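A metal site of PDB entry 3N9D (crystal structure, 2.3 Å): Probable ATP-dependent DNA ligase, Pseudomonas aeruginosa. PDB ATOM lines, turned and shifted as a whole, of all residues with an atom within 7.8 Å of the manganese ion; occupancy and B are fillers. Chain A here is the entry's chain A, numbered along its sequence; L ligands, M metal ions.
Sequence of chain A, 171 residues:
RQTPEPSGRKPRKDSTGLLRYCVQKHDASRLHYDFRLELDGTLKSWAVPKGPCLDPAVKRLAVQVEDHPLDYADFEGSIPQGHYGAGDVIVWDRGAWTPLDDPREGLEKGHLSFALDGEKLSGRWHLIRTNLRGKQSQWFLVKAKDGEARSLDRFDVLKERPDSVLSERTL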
ATOM      1  N   GLN A  24     -14.257   5.458  -4.499  1.00  0.00           N
ATOM      2  CA  GLN A  24     -14.385   6.669  -5.286  1.00  0.00           C
ATOM      3  C   GLN A  24     -13.650   7.832  -4.646  1.00  0.00           C
ATOM      4  O   GLN A  24     -13.772   8.064  -3.440  1.00  0.00           O
ATOM      5  CB  GLN A  24     -15.866   7.030  -5.489  1.00  0.00           C
ATOM      6  CG  GLN A  24     -16.544   6.214  -6.569  1.00  0.00           C
ATOM      7  CD  GLN A  24     -18.048   6.436  -6.599  1.00  0.00           C
ATOM      8  OE1 GLN A  24     -18.687   6.558  -5.545  1.00  0.00           O
ATOM      9  NE2 GLN A  24     -18.620   6.477  -7.793  1.00  0.00           N
ATOM     10  N   LYS A  25     -12.882   8.543  -5.456  1.00  0.00           N
ATOM     11  CA  LYS A  25     -12.185   9.732  -4.989  1.00  0.00           C
ATOM     12  C   LYS A  25     -13.070  10.931  -5.247  1.00  0.00           C
ATOM     13  O   LYS A  25     -13.279  11.328  -6.394  1.00  0.00           O
ATOM     14  CB  LYS A  25     -10.841   9.874  -5.718  1.00  0.00           C
ATOM     15  CG  LYS A  25     -10.018  11.088  -5.306  1.00  0.00           C
ATOM     16  CD  LYS A  25      -8.602  10.965  -5.848  1.00  0.00           C
ATOM     17  CE  LYS A  25      -7.938  12.325  -5.964  1.00  0.00           C
ATOM     18  NZ  LYS A  25      -7.940  13.058  -4.675  1.00  0.00           N
ATOM     19  N   HIS A  26     -13.618  11.500  -4.167  1.00  0.00           N
ATOM     20  CA  HIS A  26     -14.579  12.585  -4.283  1.00  0.00           C
ATOM     21  C   HIS A  26     -13.944  13.925  -3.918  1.00  0.00           C
ATOM     22  O   HIS A  26     -13.719  14.221  -2.745  1.00  0.00           O
ATOM     23  CB  HIS A  26     -15.786  12.320  -3.384  1.00  0.00           C
ATOM     24  CG  HIS A  26     -16.962  13.213  -3.674  1.00  0.00           C
ATOM     25  ND1 HIS A  26     -18.199  13.015  -3.110  1.00  0.00           N
ATOM     26  CD2 HIS A  26     -17.073  14.298  -4.482  1.00  0.00           C
ATOM     27  CE1 HIS A  26     -19.032  13.940  -3.543  1.00  0.00           C
ATOM     28  NE2 HIS A  26     -18.381  14.729  -4.375  1.00  0.00           N
ATOM     29  N   ASP A  27     -13.647  14.727  -4.933  1.00  0.00           N
ATOM     30  CA  ASP A  27     -13.030  16.029  -4.735  1.00  0.00           C
ATOM     31  C   ASP A  27     -14.071  17.080  -4.375  1.00  0.00           C
ATOM     32  O   ASP A  27     -14.338  17.999  -5.148  1.00  0.00           O
ATOM     33  CB  ASP A  27     -12.268  16.453  -6.003  1.00  0.00           C
ATOM     34  CG  ASP A  27     -11.399  17.679  -5.777  1.00  0.00           C
ATOM     35  OD1 ASP A  27     -11.306  18.146  -4.622  1.00  0.00           O
ATOM     36  OD2 ASP A  27     -10.814  18.174  -6.766  1.00  0.00           O
ATOM     37  N   ALA A  28     -14.676  16.926  -3.197  1.00  0.00           N
ATOM     38  CA  ALA A  28     -15.653  17.891  -2.708  1.00  0.00           C
ATOM     39  C   ALA A  28     -14.945  19.017  -1.985  1.00  0.00           C
ATOM     40  O   ALA A  28     -13.730  19.188  -2.118  1.00  0.00           O
ATOM     41  CB  ALA A  28     -16.660  17.208  -1.798  1.00  0.00           C
ATOM     42  N   ARG A  30     -14.067  19.231   1.006  1.00  0.00           N
ATOM     43  CA  ARG A  30     -12.940  18.548   1.635  1.00  0.00           C
ATOM     44  C   ARG A  30     -12.688  17.239   0.895  1.00  0.00           C
ATOM     45  O   ARG A  30     -13.565  16.381   0.833  1.00  0.00           O
ATOM     46  CB  ARG A  30     -13.237  18.269   3.109  1.00  0.00           C
ATOM     47  CG  ARG A  30     -13.383  19.524   3.969  1.00  0.00           C
ATOM     48  CD  ARG A  30     -12.047  20.210   4.216  1.00  0.00           C
ATOM     49  NE  ARG A  30     -11.234  19.505   5.200  1.00  0.00           N
ATOM     50  CZ  ARG A  30     -10.041  19.919   5.623  1.00  0.00           C
ATOM     51  NH1 ARG A  30      -9.519  21.044   5.145  1.00  0.00           N
ATOM     52  NH2 ARG A  30      -9.378  19.208   6.531  1.00  0.00           N
ATOM     53  N   HIS A  32     -11.791  13.577  -0.114  1.00  0.00           N
ATOM     54  CA  HIS A  32     -11.977  12.326   0.616  1.00  0.00           C
ATOM     55  C   HIS A  32     -12.253  11.159  -0.313  1.00  0.00           C
ATOM     56  O   HIS A  32     -12.481  11.340  -1.506  1.00  0.00           O
ATOM     57  CB  HIS A  32     -13.114  12.471   1.630  1.00  0.00           C
ATOM     58  CG  HIS A  32     -14.467  12.618   0.995  1.00  0.00           C
ATOM     59  ND1 HIS A  32     -14.956  13.827   0.568  1.00  0.00           N
ATOM     60  CD2 HIS A  32     -15.432  11.699   0.735  1.00  0.00           C
ATOM     61  CE1 HIS A  32     -16.168  13.651   0.061  1.00  0.00           C
ATOM     62  NE2 HIS A  32     -16.475  12.374   0.148  1.00  0.00           N
ATOM     63  N   TYR A  33     -12.231   9.947   0.240  1.00  0.00           N
ATOM     64  CA  TYR A  33     -12.456   8.739  -0.543  1.00  0.00           C
ATOM     65  C   TYR A  33     -13.696   8.014  -0.039  1.00  0.00           C
ATOM     66  O   TYR A  33     -13.895   7.850   1.157  1.00  0.00           O
ATOM     67  CB  TYR A  33     -11.241   7.814  -0.463  1.00  0.00           C
ATOM     68  CG  TYR A  33      -9.988   8.390  -1.085  1.00  0.00           C
ATOM     69  CD1 TYR A  33      -9.235   9.348  -0.429  1.00  0.00           C
ATOM     70  CD2 TYR A  33      -9.559   7.962  -2.336  1.00  0.00           C
ATOM     71  CE1 TYR A  33      -8.089   9.876  -1.001  1.00  0.00           C
ATOM     72  CE2 TYR A  33      -8.408   8.478  -2.914  1.00  0.00           C
ATOM     73  CZ  TYR A  33      -7.678   9.432  -2.235  1.00  0.00           C
ATOM     74  OH  TYR A  33      -6.548   9.952  -2.807  1.00  0.00           O
ATOM     75  N   ASP A  34     -14.531   7.576  -0.976  1.00  0.00           N
ATOM     76  CA  ASP A  34     -15.718   6.815  -0.625  1.00  0.00           C
ATOM     77  C   ASP A  34     -15.491   5.328  -0.840  1.00  0.00           C
ATOM     78  O   ASP A  34     -15.283   4.866  -1.970  1.00  0.00           O
ATOM     79  CB  ASP A  34     -16.935   7.333  -1.398  1.00  0.00           C
ATOM     80  CG  ASP A  34     -17.505   8.612  -0.806  1.00  0.00           C
ATOM     81  OD1 ASP A  34     -17.731   8.640   0.424  1.00  0.00           O
ATOM     82  OD2 ASP A  34     -17.722   9.577  -1.557  1.00  0.00           O
ATOM     83  N   ARG A  36     -16.792   1.621  -0.730  1.00  0.00           N
ATOM     84  CA  ARG A  36     -18.078   0.941  -0.857  1.00  0.00           C
ATOM     85  C   ARG A  36     -17.942  -0.581  -0.967  1.00  0.00           C
ATOM     86  O   ARG A  36     -17.078  -1.085  -1.680  1.00  0.00           O
ATOM     87  CB  ARG A  36     -18.863   1.495  -2.045  1.00  0.00           C
ATOM     88  CG  ARG A  36     -18.840   3.020  -2.136  1.00  0.00           C
ATOM     89  CD  ARG A  36     -19.856   3.528  -3.152  1.00  0.00           C
ATOM     90  NE  ARG A  36     -19.681   4.958  -3.412  1.00  0.00           N
ATOM     91  CZ  ARG A  36     -20.151   5.928  -2.637  1.00  0.00           C
ATOM     92  NH1 ARG A  36     -20.820   5.633  -1.528  1.00  0.00           N
ATOM     93  NH2 ARG A  36     -19.936   7.201  -2.958  1.00  0.00           N
ATOM     94  N   TRP A  46     -18.544   4.065   3.420  1.00  0.00           N
ATOM     95  CA  TRP A  46     -17.874   4.875   4.436  1.00  0.00           C
ATOM     96  C   TRP A  46     -17.100   5.997   3.749  1.00  0.00           C
ATOM     97  O   TRP A  46     -16.446   5.786   2.734  1.00  0.00           O
ATOM     98  CB  TRP A  46     -16.903   4.023   5.243  1.00  0.00           C
ATOM     99  CG  TRP A  46     -17.540   2.957   6.079  1.00  0.00           C
ATOM    100  CD1 TRP A  46     -17.745   2.986   7.430  1.00  0.00           C
ATOM    101  CD2 TRP A  46     -18.054   1.701   5.625  1.00  0.00           C
ATOM    102  NE1 TRP A  46     -18.344   1.824   7.842  1.00  0.00           N
ATOM    103  CE2 TRP A  46     -18.554   1.025   6.748  1.00  0.00           C
ATOM    104  CE3 TRP A  46     -18.148   1.088   4.366  1.00  0.00           C
ATOM    105  CZ2 TRP A  46     -19.130  -0.240   6.666  1.00  0.00           C
ATOM    106  CZ3 TRP A  46     -18.723  -0.166   4.283  1.00  0.00           C
ATOM    107  CH2 TRP A  46     -19.212  -0.822   5.425  1.00  0.00           C
ATOM    108  N   ALA A  47     -17.167   7.197   4.330  1.00  0.00           N
ATOM    109  CA  ALA A  47     -16.361   8.309   3.850  1.00  0.00           C
ATOM    110  C   ALA A  47     -15.017   8.336   4.573  1.00  0.00           C
ATOM    111  O   ALA A  47     -14.954   8.560   5.778  1.00  0.00           O
ATOM    112  CB  ALA A  47     -17.101   9.630   4.047  1.00  0.00           C
ATOM    113  N   VAL A  48     -13.946   8.100   3.819  1.00  0.00           N
ATOM    114  CA  VAL A  48     -12.592   8.045   4.373  1.00  0.00           C
ATOM    115  C   VAL A  48     -11.791   9.260   3.903  1.00  0.00           C
ATOM    116  O   VAL A  48     -11.218   9.257   2.822  1.00  0.00           O
ATOM    117  CB  VAL A  48     -11.866   6.757   3.923  1.00  0.00           C
ATOM    118  CG1 VAL A  48     -10.512   6.654   4.589  1.00  0.00           C
ATOM    119  CG2 VAL A  48     -12.716   5.539   4.216  1.00  0.00           C
ATOM    120  N   VAL A  65     -21.609   6.278   5.931  1.00  0.00           N
ATOM    121  CA  VAL A  65     -22.582   7.171   5.297  1.00  0.00           C
ATOM    122  C   VAL A  65     -23.700   6.390   4.617  1.00  0.00           C
ATOM    123  O   VAL A  65     -23.852   5.194   4.822  1.00  0.00           O
ATOM    124  CB  VAL A  65     -21.919   8.119   4.276  1.00  0.00           C
ATOM    125  CG1 VAL A  65     -21.010   9.110   4.991  1.00  0.00           C
ATOM    126  CG2 VAL A  65     -21.153   7.335   3.226  1.00  0.00           C
ATOM    127  N   HIS A  68     -25.579   3.266  -1.051  1.00  0.00           N
ATOM    128  CA  HIS A  68     -25.708   3.661  -2.448  1.00  0.00           C
ATOM    129  C   HIS A  68     -26.033   2.457  -3.329  1.00  0.00           C
ATOM    130  O   HIS A  68     -25.652   1.333  -3.018  1.00  0.00           O
ATOM    131  CB  HIS A  68     -24.425   4.340  -2.939  1.00  0.00           C
ATOM    132  CG  HIS A  68     -24.298   5.776  -2.516  1.00  0.00           C
ATOM    133  ND1 HIS A  68     -24.212   6.154  -1.187  1.00  0.00           N
ATOM    134  CD2 HIS A  68     -24.244   6.916  -3.233  1.00  0.00           C
ATOM    135  CE1 HIS A  68     -24.109   7.461  -1.112  1.00  0.00           C
ATOM    136  NE2 HIS A  68     -24.125   7.951  -2.336  1.00  0.00           N
ATOM    137  N   TYR A  72     -24.045   2.889  -8.876  1.00  0.00           N
ATOM    138  CA  TYR A  72     -23.300   4.102  -8.569  1.00  0.00           C
ATOM    139  C   TYR A  72     -21.816   3.801  -8.466  1.00  0.00           C
ATOM    140  O   TYR A  72     -20.981   4.700  -8.544  1.00  0.00           O
ATOM    141  CB  TYR A  72     -23.800   4.760  -7.281  1.00  0.00           C
ATOM    142  CG  TYR A  72     -23.280   6.175  -7.123  1.00  0.00           C
ATOM    143  CD1 TYR A  72     -23.807   7.219  -7.872  1.00  0.00           C
ATOM    144  CD2 TYR A  72     -22.247   6.464  -6.235  1.00  0.00           C
ATOM    145  CE1 TYR A  72     -23.335   8.505  -7.741  1.00  0.00           C
ATOM    146  CE2 TYR A  72     -21.759   7.760  -6.092  1.00  0.00           C
ATOM    147  CZ  TYR A  72     -22.311   8.777  -6.845  1.00  0.00           C
ATOM    148  OH  TYR A  72     -21.854  10.066  -6.714  1.00  0.00           O
ATOM    149  N   ILE A  79     -20.957  16.010  -8.610  1.00  0.00           N
ATOM    150  CA  ILE A  79     -22.049  16.299  -7.691  1.00  0.00           C
ATOM    151  C   ILE A  79     -22.301  17.803  -7.720  1.00  0.00           C
ATOM    152  O   ILE A  79     -21.408  18.589  -7.380  1.00  0.00           O
ATOM    153  CB  ILE A  79     -21.715  15.844  -6.261  1.00  0.00           C
ATOM    154  CG1 ILE A  79     -21.217  14.401  -6.263  1.00  0.00           C
ATOM    155  CG2 ILE A  79     -22.927  16.008  -5.355  1.00  0.00           C
ATOM    156  CD1 ILE A  79     -22.228  13.400  -6.762  1.00  0.00           C
ATOM    157  N   ALA A  86     -19.719  17.379  -3.642  1.00  0.00           N
ATOM    158  CA  ALA A  86     -20.221  18.583  -4.296  1.00  0.00           C
ATOM    159  C   ALA A  86     -19.248  19.037  -5.377  1.00  0.00           C
ATOM    160  O   ALA A  86     -19.522  20.004  -6.099  1.00  0.00           O
ATOM    161  CB  ALA A  86     -20.450  19.687  -3.275  1.00  0.00           C
ATOM    162  N   VAL A  89     -16.151  13.438  -9.169  1.00  0.00           N
ATOM    163  CA  VAL A  89     -15.906  12.096  -8.646  1.00  0.00           C
ATOM    164  C   VAL A  89     -15.319  11.176  -9.706  1.00  0.00           C
ATOM    165  O   VAL A  89     -15.756  11.171 -10.854  1.00  0.00           O
ATOM    166  CB  VAL A  89     -17.233  11.454  -8.165  1.00  0.00           C
ATOM    167  CG1 VAL A  89     -17.028   9.983  -7.833  1.00  0.00           C
ATOM    168  CG2 VAL A  89     -17.809  12.222  -6.995  1.00  0.00           C
HETATM  169  S1  LIG L   1     -21.844  11.646  -1.502  1.00  0.00           S
HETATM  170  O1  LIG L   1     -21.823  12.875  -0.726  1.00  0.00           O
HETATM  171  O2  LIG L   1     -22.390  11.942  -2.825  1.00  0.00           O
HETATM  172  O3  LIG L   1     -20.497  11.099  -1.667  1.00  0.00           O
HETATM  173  O4  LIG L   1     -22.675  10.663  -0.823  1.00  0.00           O
HETATM  174 MN    MN M   1     -18.516  11.811  -0.860  1.00  0.00          MN
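O3 of the ligand is bound to the manganese ion (2.3 Å). NE2 of His 32 is bound to the manganese ion, at 2.3 Å. The side-chain carboxylate (OD2) of Asp 34 binds the manganese ion (2.5 Å). A ring nitrogen (ND1) of His 26 binds the manganese ion (2.6 Å). The manganese ion has four donor atoms within binding distance.
NE2 of His 26 sits at hydrogen-bond distance from N of Ala 86 (3.1 Å). O of Gln 24 is in hydrogen-bond range of N of Asp 34, at 2.6 Å. The backbone carbonyl oxygen (O) of Arg 30 lies within hydrogen-bond range of a ring nitrogen (ND1) of His 32, at 2.9 Å. The side-chain carboxylate (OD2) of Asp 34 sits close to the guanidinium group (NH2) of Arg 36 (3.5 Å).
Three residues have an atom within 4 Å of the manganese ion: His 26, His 32 and Asp 34. Along chain A the residues within 4 Å of the manganese ion span positions 26 to 34.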
